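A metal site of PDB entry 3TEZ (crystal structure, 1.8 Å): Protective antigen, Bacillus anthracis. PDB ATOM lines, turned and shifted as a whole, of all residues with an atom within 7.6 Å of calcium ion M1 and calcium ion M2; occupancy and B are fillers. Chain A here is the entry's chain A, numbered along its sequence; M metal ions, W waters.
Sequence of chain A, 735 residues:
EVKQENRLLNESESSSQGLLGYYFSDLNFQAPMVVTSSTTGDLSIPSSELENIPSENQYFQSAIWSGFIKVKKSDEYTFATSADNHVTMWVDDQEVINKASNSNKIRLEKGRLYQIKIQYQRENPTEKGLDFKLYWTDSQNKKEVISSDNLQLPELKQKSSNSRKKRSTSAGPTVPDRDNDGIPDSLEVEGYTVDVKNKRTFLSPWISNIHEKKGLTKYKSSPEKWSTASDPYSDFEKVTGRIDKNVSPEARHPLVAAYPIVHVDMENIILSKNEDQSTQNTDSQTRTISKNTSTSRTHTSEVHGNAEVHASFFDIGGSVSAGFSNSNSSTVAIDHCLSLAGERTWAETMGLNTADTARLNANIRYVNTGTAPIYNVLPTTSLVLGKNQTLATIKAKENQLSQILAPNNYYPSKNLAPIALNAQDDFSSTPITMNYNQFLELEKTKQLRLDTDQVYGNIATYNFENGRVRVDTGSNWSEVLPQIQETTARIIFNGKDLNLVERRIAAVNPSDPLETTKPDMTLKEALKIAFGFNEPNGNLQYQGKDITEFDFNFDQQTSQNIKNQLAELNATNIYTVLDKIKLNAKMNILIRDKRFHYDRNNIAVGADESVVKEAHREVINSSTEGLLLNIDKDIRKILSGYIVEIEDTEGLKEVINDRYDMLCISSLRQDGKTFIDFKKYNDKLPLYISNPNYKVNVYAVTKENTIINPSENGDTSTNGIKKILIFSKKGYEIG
The side-chain hydroxyl (OG) of Ser 222 is in hydrogen-bond range of the backbone NH (N) of Lys 225 (3.2 Å). The side-chain hydroxyl (OG) of Ser 222 sits at hydrogen-bond distance from the backbone NH (N) of Glu 224, at 3.0 Å. The backbone carbonyl oxygen (O) of Glu 188 is in hydrogen-bond range of the backbone NH (N) of Ser 221 (2.9 Å). O of Pro 223 sits close to N of Asp 179 (3.3 Å). N of Asp 235 lies within hydrogen-bond range of O of Trp 226 (2.9 Å). The backbone NH of Gly 182 is in hydrogen-bond range of the side-chain carboxylate of Asp 177. The backbone NH (N) of Asp 177 sits close to the side-chain carboxylate (OD1) of Asp 185 (3.3 Å). The side-chain amino group (NZ) of Lys 225 is in hydrogen-bond range of the backbone carbonyl oxygen (O) of Thr 228.
Thr 228 touches calcium ion M1 (OG1 to CA, 3.96 Å). Of the 26 residues printed, 7 come within 4 Å of calcium ion M1.
Of the 26 residues printed, 5 come within 4 Å of calcium ion M2. The nearest printed residue that does not touch calcium ion M2 is Pro 223 (4.3 Å).
Calcium ion M1 is bound by O of Ser 222, OE1 of Glu 188, OD2 of Asp 181, OD2 of Asp 179, OD2 of Asp 235, O of Lys 225 and OE2 of Glu 188. Calcium ion M1 has seven donor atoms within binding distance.
The backbone carbonyl oxygen (O) of Ile 183 is bound to calcium ion M2 (2.3 Å). OE2 of Glu 188 is bound to calcium ion M2 (2.4 Å). The side-chain carboxylate (OD1) of Asp 179 binds calcium ion M2 (2.4 Å). OD1 of Asp 177 binds calcium ion M2, 2.4 Å away. Water W1 binds calcium ion M2 (2.4 Å). Calcium ion M2 is bound by OD1 of Asp 181 (2.5 Å). Calcium ion M2 has six donor atoms within binding distance.
Water W1 lies within hydrogen-bond range of OD1 of Asp 185 (2.5 Å), O of Pro 223 (2.6 Å) and N of Arg 178 (3.4 Å).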
ATOM      1  N   TYR A  22       6.084 -21.770 -10.261  1.00  0.00           N
ATOM      2  CA  TYR A  22       6.195 -21.158 -11.576  1.00  0.00           C
ATOM      3  C   TYR A  22       6.632 -22.234 -12.561  1.00  0.00           C
ATOM      4  O   TYR A  22       7.650 -22.875 -12.340  1.00  0.00           O
ATOM      5  CB  TYR A  22       7.247 -20.049 -11.545  1.00  0.00           C
ATOM      6  CG  TYR A  22       6.897 -18.928 -10.577  1.00  0.00           C
ATOM      7  CD1 TYR A  22       7.385 -18.929  -9.289  1.00  0.00           C
ATOM      8  CD2 TYR A  22       6.055 -17.897 -10.965  1.00  0.00           C
ATOM      9  CE1 TYR A  22       7.072 -17.923  -8.409  1.00  0.00           C
ATOM     10  CE2 TYR A  22       5.724 -16.885 -10.078  1.00  0.00           C
ATOM     11  CZ  TYR A  22       6.241 -16.906  -8.815  1.00  0.00           C
ATOM     12  OH  TYR A  22       5.931 -15.901  -7.926  1.00  0.00           O
ATOM     13  N   PRO A 176      11.969 -12.747 -12.151  1.00  0.00           N
ATOM     14  CA  PRO A 176      11.760 -11.309 -11.949  1.00  0.00           C
ATOM     15  C   PRO A 176      10.371 -11.026 -11.351  1.00  0.00           C
ATOM     16  O   PRO A 176       9.361 -11.400 -11.937  1.00  0.00           O
ATOM     17  CB  PRO A 176      11.886 -10.741 -13.376  1.00  0.00           C
ATOM     18  CG  PRO A 176      12.749 -11.749 -14.106  1.00  0.00           C
ATOM     19  CD  PRO A 176      12.350 -13.082 -13.532  1.00  0.00           C
ATOM     20  N   ASP A 177      10.364 -10.420 -10.173  1.00  0.00           N
ATOM     21  CA  ASP A 177       9.114 -10.050  -9.484  1.00  0.00           C
ATOM     22  C   ASP A 177       9.432  -8.802  -8.676  1.00  0.00           C
ATOM     23  O   ASP A 177       9.524  -8.866  -7.457  1.00  0.00           O
ATOM     24  CB  ASP A 177       8.672 -11.190  -8.565  1.00  0.00           C
ATOM     25  CG  ASP A 177       7.329 -10.914  -7.888  1.00  0.00           C
ATOM     26  OD1 ASP A 177       6.614  -9.988  -8.324  1.00  0.00           O
ATOM     27  OD2 ASP A 177       6.982 -11.602  -6.906  1.00  0.00           O
ATOM     28  N   ARG A 178       9.624  -7.690  -9.368  1.00  0.00           N
ATOM     29  CA  ARG A 178      10.149  -6.442  -8.785  1.00  0.00           C
ATOM     30  C   ARG A 178       9.347  -5.948  -7.557  1.00  0.00           C
ATOM     31  O   ARG A 178       9.920  -5.448  -6.588  1.00  0.00           O
ATOM     32  CB  ARG A 178      10.266  -5.364  -9.891  1.00  0.00           C
ATOM     33  CG  ARG A 178      11.240  -5.752 -11.017  1.00  0.00           C
ATOM     34  CD  ARG A 178      11.139  -4.849 -12.250  1.00  0.00           C
ATOM     35  NE  ARG A 178      11.888  -3.597 -12.106  1.00  0.00           N
ATOM     36  CZ  ARG A 178      13.205  -3.495 -12.182  1.00  0.00           C
ATOM     37  NH1 ARG A 178      13.944  -4.586 -12.375  1.00  0.00           N
ATOM     38  NH2 ARG A 178      13.797  -2.316 -12.053  1.00  0.00           N
ATOM     39  N   ASP A 179       8.026  -6.130  -7.580  1.00  0.00           N
ATOM     40  CA  ASP A 179       7.188  -5.640  -6.480  1.00  0.00           C
ATOM     41  C   ASP A 179       6.808  -6.710  -5.453  1.00  0.00           C
ATOM     42  O   ASP A 179       6.077  -6.441  -4.511  1.00  0.00           O
ATOM     43  CB  ASP A 179       5.909  -4.983  -7.030  1.00  0.00           C
ATOM     44  CG  ASP A 179       5.136  -5.903  -7.937  1.00  0.00           C
ATOM     45  OD1 ASP A 179       5.359  -7.134  -7.880  1.00  0.00           O
ATOM     46  OD2 ASP A 179       4.344  -5.371  -8.738  1.00  0.00           O
ATOM     47  N   ASN A 180       7.307  -7.931  -5.626  1.00  0.00           N
ATOM     48  CA  ASN A 180       7.045  -8.997  -4.667  1.00  0.00           C
ATOM     49  C   ASN A 180       5.574  -9.356  -4.518  1.00  0.00           C
ATOM     50  O   ASN A 180       5.146  -9.799  -3.439  1.00  0.00           O
ATOM     51  CB  ASN A 180       7.664  -8.698  -3.282  1.00  0.00           C
ATOM     52  CG  ASN A 180       7.904  -9.962  -2.440  1.00  0.00           C
ATOM     53  OD1 ASN A 180       8.475 -10.980  -3.076  1.00  0.00           O
ATOM     54  ND2 ASN A 180       7.576 -10.029  -1.260  1.00  0.00           N
ATOM     55  N   ASP A 181       4.768  -9.181  -5.572  1.00  0.00           N
ATOM     56  CA  ASP A 181       3.366  -9.577  -5.370  1.00  0.00           C
ATOM     57  C   ASP A 181       3.145 -11.031  -5.773  1.00  0.00           C
ATOM     58  O   ASP A 181       2.104 -11.616  -5.477  1.00  0.00           O
ATOM     59  CB  ASP A 181       2.356  -8.627  -6.043  1.00  0.00           C
ATOM     60  CG  ASP A 181       2.506  -8.550  -7.543  1.00  0.00           C
ATOM     61  OD1 ASP A 181       3.112  -9.453  -8.184  1.00  0.00           O
ATOM     62  OD2 ASP A 181       1.952  -7.580  -8.112  1.00  0.00           O
ATOM     63  N   GLY A 182       4.140 -11.612  -6.417  1.00  0.00           N
ATOM     64  CA  GLY A 182       4.037 -13.000  -6.834  1.00  0.00           C
ATOM     65  C   GLY A 182       3.812 -13.187  -8.316  1.00  0.00           C
ATOM     66  O   GLY A 182       4.032 -14.269  -8.843  1.00  0.00           O
ATOM     67  N   ILE A 183       3.358 -12.151  -9.012  1.00  0.00           N
ATOM     68  CA  ILE A 183       3.176 -12.248 -10.463  1.00  0.00           C
ATOM     69  C   ILE A 183       4.441 -11.789 -11.156  1.00  0.00           C
ATOM     70  O   ILE A 183       4.869 -10.651 -10.978  1.00  0.00           O
ATOM     71  CB  ILE A 183       1.982 -11.421 -10.974  1.00  0.00           C
ATOM     72  CG1 ILE A 183       0.710 -11.683 -10.135  1.00  0.00           C
ATOM     73  CG2 ILE A 183       1.775 -11.687 -12.509  1.00  0.00           C
ATOM     74  CD1 ILE A 183      -0.474 -10.719 -10.397  1.00  0.00           C
ATOM     75  N   PRO A 184       5.058 -12.658 -11.970  1.00  0.00           N
ATOM     76  CA  PRO A 184       6.308 -12.329 -12.679  1.00  0.00           C
ATOM     77  C   PRO A 184       6.186 -11.033 -13.487  1.00  0.00           C
ATOM     78  O   PRO A 184       5.143 -10.803 -14.096  1.00  0.00           O
ATOM     79  CB  PRO A 184       6.489 -13.521 -13.614  1.00  0.00           C
ATOM     80  CG  PRO A 184       5.793 -14.662 -12.898  1.00  0.00           C
ATOM     81  CD  PRO A 184       4.600 -14.024 -12.251  1.00  0.00           C
ATOM     82  N   ASP A 185       7.234 -10.205 -13.515  1.00  0.00           N
ATOM     83  CA  ASP A 185       7.198  -8.940 -14.264  1.00  0.00           C
ATOM     84  C   ASP A 185       6.574  -9.100 -15.656  1.00  0.00           C
ATOM     85  O   ASP A 185       5.735  -8.302 -16.075  1.00  0.00           O
ATOM     86  CB  ASP A 185       8.606  -8.376 -14.494  1.00  0.00           C
ATOM     87  CG  ASP A 185       9.337  -8.016 -13.208  1.00  0.00           C
ATOM     88  OD1 ASP A 185       8.814  -8.205 -12.091  1.00  0.00           O
ATOM     89  OD2 ASP A 185      10.503  -7.553 -13.347  1.00  0.00           O
ATOM     90  N   SER A 186       7.034 -10.098 -16.397  1.00  0.00           N
ATOM     91  CA  SER A 186       6.665 -10.239 -17.801  1.00  0.00           C
ATOM     92  C   SER A 186       5.167 -10.450 -17.988  1.00  0.00           C
ATOM     93  O   SER A 186       4.586  -9.953 -18.956  1.00  0.00           O
ATOM     94  CB  SER A 186       7.453 -11.361 -18.488  1.00  0.00           C
ATOM     95  OG  SER A 186       7.198 -12.616 -17.904  1.00  0.00           O
ATOM     96  N   GLU A 188       2.741  -9.400 -15.921  1.00  0.00           N
ATOM     97  CA  GLU A 188       1.993  -8.196 -15.552  1.00  0.00           C
ATOM     98  C   GLU A 188       1.985  -7.189 -16.707  1.00  0.00           C
ATOM     99  O   GLU A 188       0.989  -6.502 -16.962  1.00  0.00           O
ATOM    100  CB  GLU A 188       2.585  -7.554 -14.293  1.00  0.00           C
ATOM    101  CG  GLU A 188       2.388  -8.357 -13.031  1.00  0.00           C
ATOM    102  CD  GLU A 188       2.450  -7.524 -11.787  1.00  0.00           C
ATOM    103  OE1 GLU A 188       1.512  -6.737 -11.513  1.00  0.00           O
ATOM    104  OE2 GLU A 188       3.441  -7.624 -11.057  1.00  0.00           O
ATOM    105  N   TYR A 192      -2.157 -11.213 -18.704  1.00  0.00           N
ATOM    106  CA  TYR A 192      -2.372 -12.534 -18.137  1.00  0.00           C
ATOM    107  C   TYR A 192      -3.854 -12.818 -17.916  1.00  0.00           C
ATOM    108  O   TYR A 192      -4.694 -11.909 -17.889  1.00  0.00           O
ATOM    109  CB  TYR A 192      -1.614 -12.724 -16.804  1.00  0.00           C
ATOM    110  CG  TYR A 192      -1.870 -11.670 -15.733  1.00  0.00           C
ATOM    111  CD1 TYR A 192      -1.255 -10.429 -15.798  1.00  0.00           C
ATOM    112  CD2 TYR A 192      -2.684 -11.939 -14.643  1.00  0.00           C
ATOM    113  CE1 TYR A 192      -1.459  -9.475 -14.819  1.00  0.00           C
ATOM    114  CE2 TYR A 192      -2.913 -10.987 -13.643  1.00  0.00           C
ATOM    115  CZ  TYR A 192      -2.289  -9.748 -13.734  1.00  0.00           C
ATOM    116  OH  TYR A 192      -2.484  -8.786 -12.768  1.00  0.00           O
ATOM    117  N   SER A 221      -1.080  -5.307 -15.243  1.00  0.00           N
ATOM    118  CA  SER A 221      -0.878  -4.575 -13.997  1.00  0.00           C
ATOM    119  C   SER A 221       0.574  -4.067 -13.970  1.00  0.00           C
ATOM    120  O   SER A 221       1.357  -4.431 -14.829  1.00  0.00           O
ATOM    121  CB  SER A 221      -1.206  -5.467 -12.807  1.00  0.00           C
ATOM    122  OG  SER A 221      -0.631  -6.768 -12.958  1.00  0.00           O
ATOM    123  N   SER A 222       0.910  -3.211 -13.018  1.00  0.00           N
ATOM    124  CA  SER A 222       2.283  -2.720 -12.951  1.00  0.00           C
ATOM    125  C   SER A 222       3.182  -3.729 -12.254  1.00  0.00           C
ATOM    126  O   SER A 222       2.857  -4.174 -11.174  1.00  0.00           O
ATOM    127  CB  SER A 222       2.396  -1.412 -12.181  1.00  0.00           C
ATOM    128  OG  SER A 222       3.788  -1.178 -11.915  1.00  0.00           O
ATOM    129  N   PRO A 223       4.326  -4.065 -12.872  1.00  0.00           N
ATOM    130  CA  PRO A 223       5.299  -4.980 -12.255  1.00  0.00           C
ATOM    131  C   PRO A 223       6.091  -4.329 -11.118  1.00  0.00           C
ATOM    132  O   PRO A 223       6.850  -5.003 -10.438  1.00  0.00           O
ATOM    133  CB  PRO A 223       6.217  -5.347 -13.420  1.00  0.00           C
ATOM    134  CG  PRO A 223       6.197  -4.135 -14.294  1.00  0.00           C
ATOM    135  CD  PRO A 223       4.752  -3.645 -14.216  1.00  0.00           C
ATOM    136  N   GLU A 224       5.861  -3.032 -10.888  1.00  0.00           N
ATOM    137  CA  GLU A 224       6.572  -2.308  -9.826  1.00  0.00           C
ATOM    138  C   GLU A 224       5.641  -1.744  -8.731  1.00  0.00           C
ATOM    139  O   GLU A 224       6.087  -1.106  -7.762  1.00  0.00           O
ATOM    140  CB  GLU A 224       7.449  -1.232 -10.452  1.00  0.00           C
ATOM    141  CG  GLU A 224       8.553  -1.841 -11.341  1.00  0.00           C
ATOM    142  CD  GLU A 224       9.501  -0.812 -11.927  1.00  0.00           C
ATOM    143  OE1 GLU A 224       9.490   0.337 -11.440  1.00  0.00           O
ATOM    144  OE2 GLU A 224      10.251  -1.150 -12.878  1.00  0.00           O
ATOM    145  N   LYS A 225       4.349  -2.016  -8.879  1.00  0.00           N
ATOM    146  CA  LYS A 225       3.400  -1.688  -7.828  1.00  0.00           C
ATOM    147  C   LYS A 225       2.759  -2.967  -7.321  1.00  0.00           C
ATOM    148  O   LYS A 225       2.060  -3.643  -8.063  1.00  0.00           O
ATOM    149  CB  LYS A 225       2.334  -0.744  -8.370  1.00  0.00           C
ATOM    150  CG  LYS A 225       2.888   0.546  -8.949  1.00  0.00           C
ATOM    151  CD  LYS A 225       1.749   1.518  -9.293  1.00  0.00           C
ATOM    152  CE  LYS A 225       1.137   2.137  -8.043  1.00  0.00           C
ATOM    153  NZ  LYS A 225      -0.040   2.934  -8.446  1.00  0.00           N
ATOM    154  N   TRP A 226       2.994  -3.283  -6.062  1.00  0.00           N
ATOM    155  CA  TRP A 226       2.441  -4.460  -5.410  1.00  0.00           C
ATOM    156  C   TRP A 226       0.905  -4.439  -5.519  1.00  0.00           C
ATOM    157  O   TRP A 226       0.290  -5.455  -5.840  1.00  0.00           O
ATOM    158  CB  TRP A 226       2.932  -4.468  -3.960  1.00  0.00           C
ATOM    159  CG  TRP A 226       2.407  -5.537  -3.049  1.00  0.00           C
ATOM    160  CD1 TRP A 226       2.945  -6.775  -2.825  1.00  0.00           C
ATOM    161  CD2 TRP A 226       1.268  -5.433  -2.179  1.00  0.00           C
ATOM    162  NE1 TRP A 226       2.195  -7.461  -1.899  1.00  0.00           N
ATOM    163  CE2 TRP A 226       1.156  -6.656  -1.483  1.00  0.00           C
ATOM    164  CE3 TRP A 226       0.310  -4.437  -1.947  1.00  0.00           C
ATOM    165  CZ2 TRP A 226       0.142  -6.914  -0.561  1.00  0.00           C
ATOM    166  CZ3 TRP A 226      -0.706  -4.684  -1.012  1.00  0.00           C
ATOM    167  CH2 TRP A 226      -0.787  -5.917  -0.342  1.00  0.00           C
ATOM    168  N   SER A 227       0.295  -3.289  -5.237  1.00  0.00           N
ATOM    169  CA  SER A 227      -1.100  -3.032  -5.635  1.00  0.00           C
ATOM    170  C   SER A 227      -1.074  -1.935  -6.678  1.00  0.00           C
ATOM    171  O   SER A 227      -0.651  -0.810  -6.403  1.00  0.00           O
ATOM    172  CB  SER A 227      -1.970  -2.607  -4.457  1.00  0.00           C
ATOM    173  OG  SER A 227      -3.246  -2.177  -4.916  1.00  0.00           O
ATOM    174  N   THR A 228      -1.514  -2.261  -7.879  1.00  0.00           N
ATOM    175  CA  THR A 228      -1.434  -1.307  -8.980  1.00  0.00           C
ATOM    176  C   THR A 228      -2.404  -0.127  -8.777  1.00  0.00           C
ATOM    177  O   THR A 228      -2.106   0.991  -9.195  1.00  0.00           O
ATOM    178  CB  THR A 228      -1.626  -2.008 -10.323  1.00  0.00           C
ATOM    179  OG1 THR A 228      -0.507  -2.879 -10.543  1.00  0.00           O
ATOM    180  CG2 THR A 228      -1.704  -1.010 -11.473  1.00  0.00           C
ATOM    181  N   SER A 234      -3.028  -6.913  -2.865  1.00  0.00           N
ATOM    182  CA  SER A 234      -2.051  -7.049  -3.938  1.00  0.00           C
ATOM    183  C   SER A 234      -2.666  -7.521  -5.268  1.00  0.00           C
ATOM    184  O   SER A 234      -3.751  -8.133  -5.297  1.00  0.00           O
ATOM    185  CB  SER A 234      -0.925  -7.997  -3.541  1.00  0.00           C
ATOM    186  OG  SER A 234      -1.133  -9.282  -4.083  1.00  0.00           O
ATOM    187  N   ASP A 235      -1.976  -7.242  -6.361  1.00  0.00           N
ATOM    188  CA  ASP A 235      -2.484  -7.635  -7.687  1.00  0.00           C
ATOM    189  C   ASP A 235      -2.751  -9.150  -7.722  1.00  0.00           C
ATOM    190  O   ASP A 235      -3.742  -9.627  -8.268  1.00  0.00           O
ATOM    191  CB  ASP A 235      -1.510  -7.220  -8.783  1.00  0.00           C
ATOM    192  CG  ASP A 235      -1.340  -5.731  -8.867  1.00  0.00           C
ATOM    193  OD1 ASP A 235      -2.232  -4.955  -8.460  1.00  0.00           O
ATOM    194  OD2 ASP A 235      -0.295  -5.308  -9.390  1.00  0.00           O
ATOM    195  N   PHE A 236      -1.855  -9.901  -7.089  1.00  0.00           N
ATOM    196  CA  PHE A 236      -1.975 -11.354  -6.997  1.00  0.00           C
ATOM    197  C   PHE A 236      -3.077 -11.805  -6.030  1.00  0.00           C
ATOM    198  O   PHE A 236      -3.854 -12.723  -6.346  1.00  0.00           O
ATOM    199  CB  PHE A 236      -0.599 -11.901  -6.587  1.00  0.00           C
ATOM    200  CG  PHE A 236      -0.554 -13.394  -6.383  1.00  0.00           C
ATOM    201  CD1 PHE A 236      -0.423 -14.246  -7.469  1.00  0.00           C
ATOM    202  CD2 PHE A 236      -0.609 -13.928  -5.100  1.00  0.00           C
ATOM    203  CE1 PHE A 236      -0.335 -15.625  -7.274  1.00  0.00           C
ATOM    204  CE2 PHE A 236      -0.533 -15.304  -4.910  1.00  0.00           C
ATOM    205  CZ  PHE A 236      -0.402 -16.156  -5.995  1.00  0.00           C
ATOM    206  N   PRO A 254      -6.982  -5.871 -10.832  1.00  0.00           N
ATOM    207  CA  PRO A 254      -5.851  -5.091 -10.322  1.00  0.00           C
ATOM    208  C   PRO A 254      -5.880  -3.608 -10.709  1.00  0.00           C
ATOM    209  O   PRO A 254      -5.178  -2.825 -10.059  1.00  0.00           O
ATOM    210  CB  PRO A 254      -4.633  -5.780 -10.955  1.00  0.00           C
ATOM    211  CG  PRO A 254      -5.067  -7.189 -11.177  1.00  0.00           C
ATOM    212  CD  PRO A 254      -6.536  -7.087 -11.549  1.00  0.00           C
HETATM  213 CA    CA M   1       2.109  -5.660  -9.503  1.00  0.00          CA
HETATM  214 CA    CA M   2       4.978  -8.759  -9.657  1.00  0.00          CA
HETATM  215  O   HOH W   1       6.649  -7.517 -10.945  1.00  0.00           O
